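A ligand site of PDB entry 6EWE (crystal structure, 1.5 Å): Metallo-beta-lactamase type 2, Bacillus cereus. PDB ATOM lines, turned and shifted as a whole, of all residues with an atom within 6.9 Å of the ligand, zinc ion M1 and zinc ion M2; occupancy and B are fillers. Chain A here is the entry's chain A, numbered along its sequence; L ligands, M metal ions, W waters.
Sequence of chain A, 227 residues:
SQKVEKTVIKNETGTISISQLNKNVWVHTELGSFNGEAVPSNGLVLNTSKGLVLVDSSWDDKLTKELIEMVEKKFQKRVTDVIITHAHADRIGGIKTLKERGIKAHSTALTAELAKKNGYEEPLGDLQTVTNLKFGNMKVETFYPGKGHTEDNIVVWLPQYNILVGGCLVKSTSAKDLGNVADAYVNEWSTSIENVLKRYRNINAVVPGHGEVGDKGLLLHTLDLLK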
ATOM      1  N   PRO A  40      -2.848 -16.995 -24.627  1.00  0.00           N
ATOM      2  CA  PRO A  40      -2.218 -15.790 -25.175  1.00  0.00           C
ATOM      3  C   PRO A  40      -2.011 -14.727 -24.114  1.00  0.00           C
ATOM      4  O   PRO A  40      -2.732 -14.640 -23.128  1.00  0.00           O
ATOM      5  CB  PRO A  40      -3.243 -15.304 -26.212  1.00  0.00           C
ATOM      6  CG  PRO A  40      -4.556 -15.712 -25.603  1.00  0.00           C
ATOM      7  CD  PRO A  40      -4.296 -17.030 -24.917  1.00  0.00           C
ATOM      8  N   SER A  41      -0.959 -13.936 -24.346  1.00  0.00           N
ATOM      9  CA  SER A  41      -0.554 -12.853 -23.479  1.00  0.00           C
ATOM     10  C   SER A  41      -0.221 -11.645 -24.342  1.00  0.00           C
ATOM     11  O   SER A  41       0.364 -11.802 -25.420  1.00  0.00           O
ATOM     12  CB  SER A  41       0.713 -13.292 -22.722  1.00  0.00           C
ATOM     13  OG  SER A  41       1.297 -12.226 -22.007  1.00  0.00           O
ATOM     14  N   TRP A  59       6.467 -15.341 -22.370  1.00  0.00           N
ATOM     15  CA  TRP A  59       6.375 -16.452 -21.426  1.00  0.00           C
ATOM     16  C   TRP A  59       7.737 -17.088 -21.155  1.00  0.00           C
ATOM     17  O   TRP A  59       7.943 -17.690 -20.096  1.00  0.00           O
ATOM     18  CB  TRP A  59       5.487 -17.527 -22.039  1.00  0.00           C
ATOM     19  CG  TRP A  59       4.046 -17.124 -22.214  1.00  0.00           C
ATOM     20  CD1 TRP A  59       3.463 -16.605 -23.343  1.00  0.00           C
ATOM     21  CD2 TRP A  59       3.004 -17.231 -21.234  1.00  0.00           C
ATOM     22  NE1 TRP A  59       2.118 -16.380 -23.114  1.00  0.00           N
ATOM     23  CE2 TRP A  59       1.817 -16.746 -21.832  1.00  0.00           C
ATOM     24  CE3 TRP A  59       2.965 -17.686 -19.907  1.00  0.00           C
ATOM     25  CZ2 TRP A  59       0.604 -16.727 -21.145  1.00  0.00           C
ATOM     26  CZ3 TRP A  59       1.754 -17.654 -19.240  1.00  0.00           C
ATOM     27  CH2 TRP A  59       0.591 -17.174 -19.860  1.00  0.00           C
ATOM     28  N   HIS A  86       4.699  -7.019 -13.799  1.00  0.00           N
ATOM     29  CA  HIS A  86       4.732  -7.783 -12.546  1.00  0.00           C
ATOM     30  C   HIS A  86       5.625  -9.013 -12.761  1.00  0.00           C
ATOM     31  O   HIS A  86       6.184  -9.221 -13.842  1.00  0.00           O
ATOM     32  CB  HIS A  86       3.322  -8.094 -12.054  1.00  0.00           C
ATOM     33  CG  HIS A  86       2.566  -9.103 -12.846  1.00  0.00           C
ATOM     34  ND1 HIS A  86       1.814  -8.786 -13.956  1.00  0.00           N
ATOM     35  CD2 HIS A  86       2.303 -10.397 -12.584  1.00  0.00           C
ATOM     36  CE1 HIS A  86       1.183  -9.874 -14.379  1.00  0.00           C
ATOM     37  NE2 HIS A  86       1.449 -10.861 -13.551  1.00  0.00           N
ATOM     38  N   ALA A  87       5.872  -9.757 -11.692  1.00  0.00           N
ATOM     39  CA  ALA A  87       6.869 -10.826 -11.698  1.00  0.00           C
ATOM     40  C   ALA A  87       6.321 -12.235 -12.008  1.00  0.00           C
ATOM     41  O   ALA A  87       6.853 -13.217 -11.502  1.00  0.00           O
ATOM     42  CB  ALA A  87       7.627 -10.823 -10.375  1.00  0.00           C
ATOM     43  N   HIS A  88       5.277 -12.399 -12.811  1.00  0.00           N
ATOM     44  CA  HIS A  88       4.902 -13.719 -13.306  1.00  0.00           C
ATOM     45  C   HIS A  88       5.501 -13.954 -14.693  1.00  0.00           C
ATOM     46  O   HIS A  88       5.877 -13.009 -15.374  1.00  0.00           O
ATOM     47  CB  HIS A  88       3.377 -13.790 -13.460  1.00  0.00           C
ATOM     48  CG  HIS A  88       2.603 -13.939 -12.178  1.00  0.00           C
ATOM     49  ND1 HIS A  88       1.255 -13.584 -12.059  1.00  0.00           N
ATOM     50  CD2 HIS A  88       2.948 -14.459 -10.976  1.00  0.00           C
ATOM     51  CE1 HIS A  88       0.841 -13.852 -10.832  1.00  0.00           C
ATOM     52  NE2 HIS A  88       1.838 -14.417 -10.168  1.00  0.00           N
ATOM     53  N   ALA A  89       5.500 -15.241 -15.117  1.00  0.00           N
ATOM     54  CA  ALA A  89       6.242 -15.688 -16.307  1.00  0.00           C
ATOM     55  C   ALA A  89       5.777 -15.017 -17.583  1.00  0.00           C
ATOM     56  O   ALA A  89       6.577 -14.836 -18.513  1.00  0.00           O
ATOM     57  CB  ALA A  89       6.120 -17.214 -16.495  1.00  0.00           C
ATOM     58  N   ASP A  90       4.494 -14.673 -17.677  1.00  0.00           N
ATOM     59  CA  ASP A  90       4.047 -14.049 -18.914  1.00  0.00           C
ATOM     60  C   ASP A  90       4.644 -12.682 -19.113  1.00  0.00           C
ATOM     61  O   ASP A  90       4.752 -12.228 -20.249  1.00  0.00           O
ATOM     62  CB  ASP A  90       2.513 -14.020 -19.005  1.00  0.00           C
ATOM     63  CG  ASP A  90       1.838 -13.251 -17.902  1.00  0.00           C
ATOM     64  OD1 ASP A  90       2.354 -13.181 -16.787  1.00  0.00           O
ATOM     65  OD2 ASP A  90       0.716 -12.725 -18.134  1.00  0.00           O
ATOM     66  N   ARG A  91       5.044 -12.003 -18.025  1.00  0.00           N
ATOM     67  CA  ARG A  91       5.622 -10.680 -18.087  1.00  0.00           C
ATOM     68  C   ARG A  91       7.135 -10.751 -18.115  1.00  0.00           C
ATOM     69  O   ARG A  91       7.764  -9.975 -18.822  1.00  0.00           O
ATOM     70  CB  ARG A  91       5.242  -9.841 -16.861  1.00  0.00           C
ATOM     71  CG  ARG A  91       3.724  -9.822 -16.533  1.00  0.00           C
ATOM     72  CD  ARG A  91       2.894  -9.072 -17.584  1.00  0.00           C
ATOM     73  NE  ARG A  91       2.017  -9.962 -18.323  1.00  0.00           N
ATOM     74  CZ  ARG A  91       1.424  -9.616 -19.456  1.00  0.00           C
ATOM     75  NH1 ARG A  91       1.575  -8.395 -19.903  1.00  0.00           N
ATOM     76  NH2 ARG A  91       0.653 -10.488 -20.098  1.00  0.00           N
ATOM     77  N   HIS A 149      -4.225  -8.091  -8.955  1.00  0.00           N
ATOM     78  CA  HIS A 149      -3.838  -9.383  -9.503  1.00  0.00           C
ATOM     79  C   HIS A 149      -2.615  -9.956  -8.802  1.00  0.00           C
ATOM     80  O   HIS A 149      -2.550 -11.140  -8.520  1.00  0.00           O
ATOM     81  CB  HIS A 149      -3.580  -9.220 -11.035  1.00  0.00           C
ATOM     82  CG  HIS A 149      -2.875 -10.379 -11.638  1.00  0.00           C
ATOM     83  ND1 HIS A 149      -3.470 -11.583 -11.794  1.00  0.00           N
ATOM     84  CD2 HIS A 149      -1.600 -10.519 -12.138  1.00  0.00           C
ATOM     85  CE1 HIS A 149      -2.636 -12.443 -12.338  1.00  0.00           C
ATOM     86  NE2 HIS A 149      -1.477 -11.817 -12.533  1.00  0.00           N
ATOM     87  N   THR A 150      -1.658  -9.088  -8.450  1.00  0.00           N
ATOM     88  CA  THR A 150      -0.529  -9.431  -7.632  1.00  0.00           C
ATOM     89  C   THR A 150      -0.233  -8.225  -6.787  1.00  0.00           C
ATOM     90  O   THR A 150      -0.831  -7.158  -6.920  1.00  0.00           O
ATOM     91  CB  THR A 150       0.752  -9.668  -8.451  1.00  0.00           C
ATOM     92  OG1 THR A 150       1.041  -8.506  -9.232  1.00  0.00           O
ATOM     93  CG2 THR A 150       0.713 -10.921  -9.257  1.00  0.00           C
ATOM     94  N   GLY A 167      -2.345  -4.499 -18.153  1.00  0.00           N
ATOM     95  CA  GLY A 167      -1.706  -5.706 -17.729  1.00  0.00           C
ATOM     96  C   GLY A 167      -2.725  -6.605 -17.097  1.00  0.00           C
ATOM     97  O   GLY A 167      -3.924  -6.541 -17.374  1.00  0.00           O
ATOM     98  N   CYS A 168      -2.230  -7.472 -16.204  1.00  0.00           N
ATOM     99  CA  CYS A 168      -3.056  -8.530 -15.670  1.00  0.00           C
ATOM    100  C   CYS A 168      -3.936  -8.038 -14.538  1.00  0.00           C
ATOM    101  O   CYS A 168      -4.840  -8.767 -14.160  1.00  0.00           O
ATOM    102  CB  CYS A 168      -2.170  -9.740 -15.353  1.00  0.00           C
ATOM    103  SG  CYS A 168      -1.192 -10.105 -16.844  1.00  0.00           S
ATOM    104  N   LEU A 169      -3.776  -6.773 -14.123  1.00  0.00           N
ATOM    105  CA  LEU A 169      -4.753  -6.092 -13.283  1.00  0.00           C
ATOM    106  C   LEU A 169      -6.118  -5.975 -13.962  1.00  0.00           C
ATOM    107  O   LEU A 169      -7.148  -5.899 -13.277  1.00  0.00           O
ATOM    108  CB  LEU A 169      -4.222  -4.688 -12.948  1.00  0.00           C
ATOM    109  CG  LEU A 169      -5.053  -3.870 -11.986  1.00  0.00           C
ATOM    110  CD1 LEU A 169      -4.874  -4.427 -10.548  1.00  0.00           C
ATOM    111  CD2 LEU A 169      -4.644  -2.422 -12.049  1.00  0.00           C
ATOM    112  N   LYS A 171      -8.979  -7.343 -16.655  1.00  0.00           N
ATOM    113  CA  LYS A 171      -9.490  -8.508 -17.366  1.00  0.00           C
ATOM    114  C   LYS A 171     -10.159  -8.085 -18.667  1.00  0.00           C
ATOM    115  O   LYS A 171     -10.781  -7.028 -18.745  1.00  0.00           O
ATOM    116  CB  LYS A 171     -10.513  -9.247 -16.486  1.00  0.00           C
ATOM    117  CG  LYS A 171      -9.894  -9.883 -15.260  1.00  0.00           C
ATOM    118  CD  LYS A 171      -8.930 -10.979 -15.645  1.00  0.00           C
ATOM    119  CE  LYS A 171      -8.246 -11.597 -14.445  1.00  0.00           C
ATOM    120  NZ  LYS A 171      -7.362 -12.742 -14.915  1.00  0.00           N
ATOM    121  N   LEU A 178     -11.738 -14.228 -12.383  1.00  0.00           N
ATOM    122  CA  LEU A 178     -10.503 -13.469 -12.162  1.00  0.00           C
ATOM    123  C   LEU A 178      -9.243 -14.245 -12.507  1.00  0.00           C
ATOM    124  O   LEU A 178      -8.139 -13.664 -12.456  1.00  0.00           O
ATOM    125  CB  LEU A 178     -10.457 -13.020 -10.698  1.00  0.00           C
ATOM    126  CG  LEU A 178     -11.530 -12.035 -10.285  1.00  0.00           C
ATOM    127  CD1 LEU A 178     -11.590 -11.907  -8.748  1.00  0.00           C
ATOM    128  CD2 LEU A 178     -11.295 -10.683 -10.943  1.00  0.00           C
ATOM    129  N   GLY A 179      -9.374 -15.530 -12.859  1.00  0.00           N
ATOM    130  CA  GLY A 179      -8.219 -16.382 -13.143  1.00  0.00           C
ATOM    131  C   GLY A 179      -7.576 -16.904 -11.867  1.00  0.00           C
ATOM    132  O   GLY A 179      -8.222 -17.055 -10.841  1.00  0.00           O
ATOM    133  N   ASN A 180      -6.276 -17.158 -11.937  1.00  0.00           N
ATOM    134  CA  ASN A 180      -5.536 -17.656 -10.773  1.00  0.00           C
ATOM    135  C   ASN A 180      -5.323 -16.493  -9.822  1.00  0.00           C
ATOM    136  O   ASN A 180      -4.679 -15.504 -10.174  1.00  0.00           O
ATOM    137  CB  ASN A 180      -4.207 -18.305 -11.194  1.00  0.00           C
ATOM    138  CG  ASN A 180      -3.521 -19.040 -10.028  1.00  0.00           C
ATOM    139  OD1 ASN A 180      -3.621 -18.620  -8.896  1.00  0.00           O
ATOM    140  ND2 ASN A 180      -2.828 -20.141 -10.325  1.00  0.00           N
ATOM    141  N   VAL A 181      -5.929 -16.610  -8.630  1.00  0.00           N
ATOM    142  CA  VAL A 181      -5.871 -15.587  -7.602  1.00  0.00           C
ATOM    143  C   VAL A 181      -4.935 -15.972  -6.470  1.00  0.00           C
ATOM    144  O   VAL A 181      -4.953 -15.331  -5.422  1.00  0.00           O
ATOM    145  CB  VAL A 181      -7.285 -15.220  -7.100  1.00  0.00           C
ATOM    146  CG1 VAL A 181      -8.046 -14.555  -8.231  1.00  0.00           C
ATOM    147  CG2 VAL A 181      -8.046 -16.479  -6.502  1.00  0.00           C
ATOM    148  N   ALA A 182      -4.070 -16.981  -6.672  1.00  0.00           N
ATOM    149  CA  ALA A 182      -3.172 -17.407  -5.597  1.00  0.00           C
ATOM    150  C   ALA A 182      -2.288 -16.259  -5.118  1.00  0.00           C
ATOM    151  O   ALA A 182      -1.995 -16.162  -3.912  1.00  0.00           O
ATOM    152  CB  ALA A 182      -2.294 -18.587  -6.043  1.00  0.00           C
ATOM    153  N   ASP A 183      -1.853 -15.384  -6.029  1.00  0.00           N
ATOM    154  CA  ASP A 183      -0.994 -14.265  -5.681  1.00  0.00           C
ATOM    155  C   ASP A 183      -1.760 -12.963  -5.562  1.00  0.00           C
ATOM    156  O   ASP A 183      -1.154 -11.909  -5.477  1.00  0.00           O
ATOM    157  CB  ASP A 183       0.155 -14.094  -6.711  1.00  0.00           C
ATOM    158  CG  ASP A 183       1.142 -15.248  -6.692  1.00  0.00           C
ATOM    159  OD1 ASP A 183       1.172 -16.019  -5.697  1.00  0.00           O
ATOM    160  OD2 ASP A 183       1.925 -15.355  -7.666  1.00  0.00           O
ATOM    161  N   ALA A 184      -3.107 -13.016  -5.547  1.00  0.00           N
ATOM    162  CA  ALA A 184      -3.943 -11.842  -5.706  1.00  0.00           C
ATOM    163  C   ALA A 184      -4.470 -11.333  -4.362  1.00  0.00           C
ATOM    164  O   ALA A 184      -4.408 -12.027  -3.332  1.00  0.00           O
ATOM    165  CB  ALA A 184      -5.124 -12.163  -6.629  1.00  0.00           C
ATOM    166  N   GLY A 209      -3.900  -7.748 -19.961  1.00  0.00           N
ATOM    167  CA  GLY A 209      -2.784  -8.696 -20.046  1.00  0.00           C
ATOM    168  C   GLY A 209      -3.065  -9.881 -20.950  1.00  0.00           C
ATOM    169  O   GLY A 209      -2.144 -10.442 -21.560  1.00  0.00           O
ATOM    170  N   HIS A 210      -4.314 -10.263 -21.069  1.00  0.00           N
ATOM    171  CA  HIS A 210      -4.772 -11.376 -21.893  1.00  0.00           C
ATOM    172  C   HIS A 210      -6.104 -10.973 -22.517  1.00  0.00           C
ATOM    173  O   HIS A 210      -6.984 -10.445 -21.827  1.00  0.00           O
ATOM    174  CB  HIS A 210      -4.909 -12.665 -21.049  1.00  0.00           C
ATOM    175  CG  HIS A 210      -3.707 -12.944 -20.171  1.00  0.00           C
ATOM    176  ND1 HIS A 210      -2.667 -13.741 -20.567  1.00  0.00           N
ATOM    177  CD2 HIS A 210      -3.422 -12.545 -18.899  1.00  0.00           C
ATOM    178  CE1 HIS A 210      -1.754 -13.792 -19.602  1.00  0.00           C
ATOM    179  NE2 HIS A 210      -2.199 -13.094 -18.568  1.00  0.00           N
HETATM  180  C1  LIG L   1       0.563 -16.735 -14.069  1.00  0.00           C
HETATM  181  C2  LIG L   1       0.746 -17.435 -11.688  1.00  0.00           C
HETATM  182  C3  LIG L   1       1.057 -17.869 -10.405  1.00  0.00           C
HETATM  183  C4  LIG L   1       0.180 -17.612  -9.379  1.00  0.00           C
HETATM  184  C5  LIG L   1      -1.007 -16.934  -9.623  1.00  0.00           C
HETATM  185  C6  LIG L   1      -1.331 -16.531 -10.908  1.00  0.00           C
HETATM  186  C7  LIG L   1      -0.463 -16.771 -11.974  1.00  0.00           C
HETATM  187  C8  LIG L   1      -2.972 -13.894 -15.173  1.00  0.00           C
HETATM  188  O1  LIG L   1      -4.099 -14.538 -14.863  1.00  0.00           O
HETATM  189  C9  LIG L   1      -1.721 -14.550 -14.748  1.00  0.00           C
HETATM  190  C10 LIG L   1      -1.680 -15.627 -13.916  1.00  0.00           C
HETATM  191  C11 LIG L   1      -0.555 -16.371 -13.361  1.00  0.00           C
HETATM  192  O2  LIG L   1      -2.952 -12.825 -15.712  1.00  0.00           O
HETATM  193  S1  LIG L   1      -0.212 -13.808 -15.308  1.00  0.00           S
HETATM  194  S2  LIG L   1       1.747 -17.547 -13.114  1.00  0.00           S
HETATM  195 ZN    ZN M   1      -1.074 -12.453 -16.927  1.00  0.00          ZN
HETATM  196 ZN    ZN M   2       0.251 -12.507 -13.450  1.00  0.00          ZN
HETATM  197  O   HOH W   1      -2.558 -14.054  -8.823  1.00  0.00           O
HETATM  198  O   HOH W   2      -4.964 -16.863 -14.412  1.00  0.00           O
HETATM  199  O   HOH W   3      -5.181 -11.072 -15.822  1.00  0.00           O
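O1 of the ligand is in salt-bridge range of NZ of Lys 171, at 3.7 Å.
SG of Cys 168 lies close to NE of Arg 91 (3.5 Å). A ring nitrogen (NE2) of His 88 is in hydrogen-bond range of the side-chain carboxylate of Asp 183 (2.7 Å). A ring nitrogen (ND1) of His 210 lies within hydrogen-bond range of the backbone carbonyl oxygen (O) of Pro 40, at 2.7 Å. The guanidinium group (NE) of Arg 91 lies within salt-bridge range of the side-chain carboxylate (OD1) of Asp 90 (3.6 Å). The side-chain amide oxygen of Asn 180 is in hydrogen-bond range of the backbone NH of Ala 182, 2.8 Å away. The side-chain amino group (NZ) of Lys 171 sits at hydrogen-bond distance from the backbone carbonyl oxygen (O) of Leu 178 (2.7 Å).
Residues that only touch the ligand: Asn 180 (3.2 Å) and Asp 183 (3.3 Å). Within 4 Å of the ligand: His 86, His 88, Asp 90, His 149, Cys 168, Lys 171, Asn 180, Asp 183 and His 210. The nearest printed residue that does not touch the ligand is Ala 182 (4.1 Å).
Of the 24 residues printed, 3 come within 4 Å of zinc ion M2. Along chain A the residues within 4 Å of zinc ion M2 span positions 86 to 149.
Zinc ion M1 is bound by NE2 of His 210 (2.1 Å), OD2 of Asp 90 (2.2 Å), O2 of the ligand (2.3 Å), S1 of the ligand (2.3 Å) and SG of Cys 168 (2.4 Å). Zinc ion M1 has five donor atoms within binding distance.
ND1 of His 88 is bound to zinc ion M2 (2.0 Å). A ring nitrogen (NE2) of His 86 is bound to zinc ion M2 (2.0 Å). Zinc ion M2 is bound by NE2 of His 149 (2.1 Å). S1 of the ligand binds zinc ion M2 (2.3 Å).
Water W2 bridges an oxygen (O1) of the ligand and the backbone NH (N) of Asn 180. Water W3 lies within hydrogen-bond range of the backbone carbonyl oxygen (O) of Cys 168 (2.9 Å) and the side-chain amino group (NZ) of Lys 171 (2.9 Å). Water W1 lies within hydrogen-bond range of the backbone carbonyl oxygen of Asn 180, the backbone carbonyl oxygen of His 149, the backbone NH of Asp 183 and the backbone NH of Ala 184.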
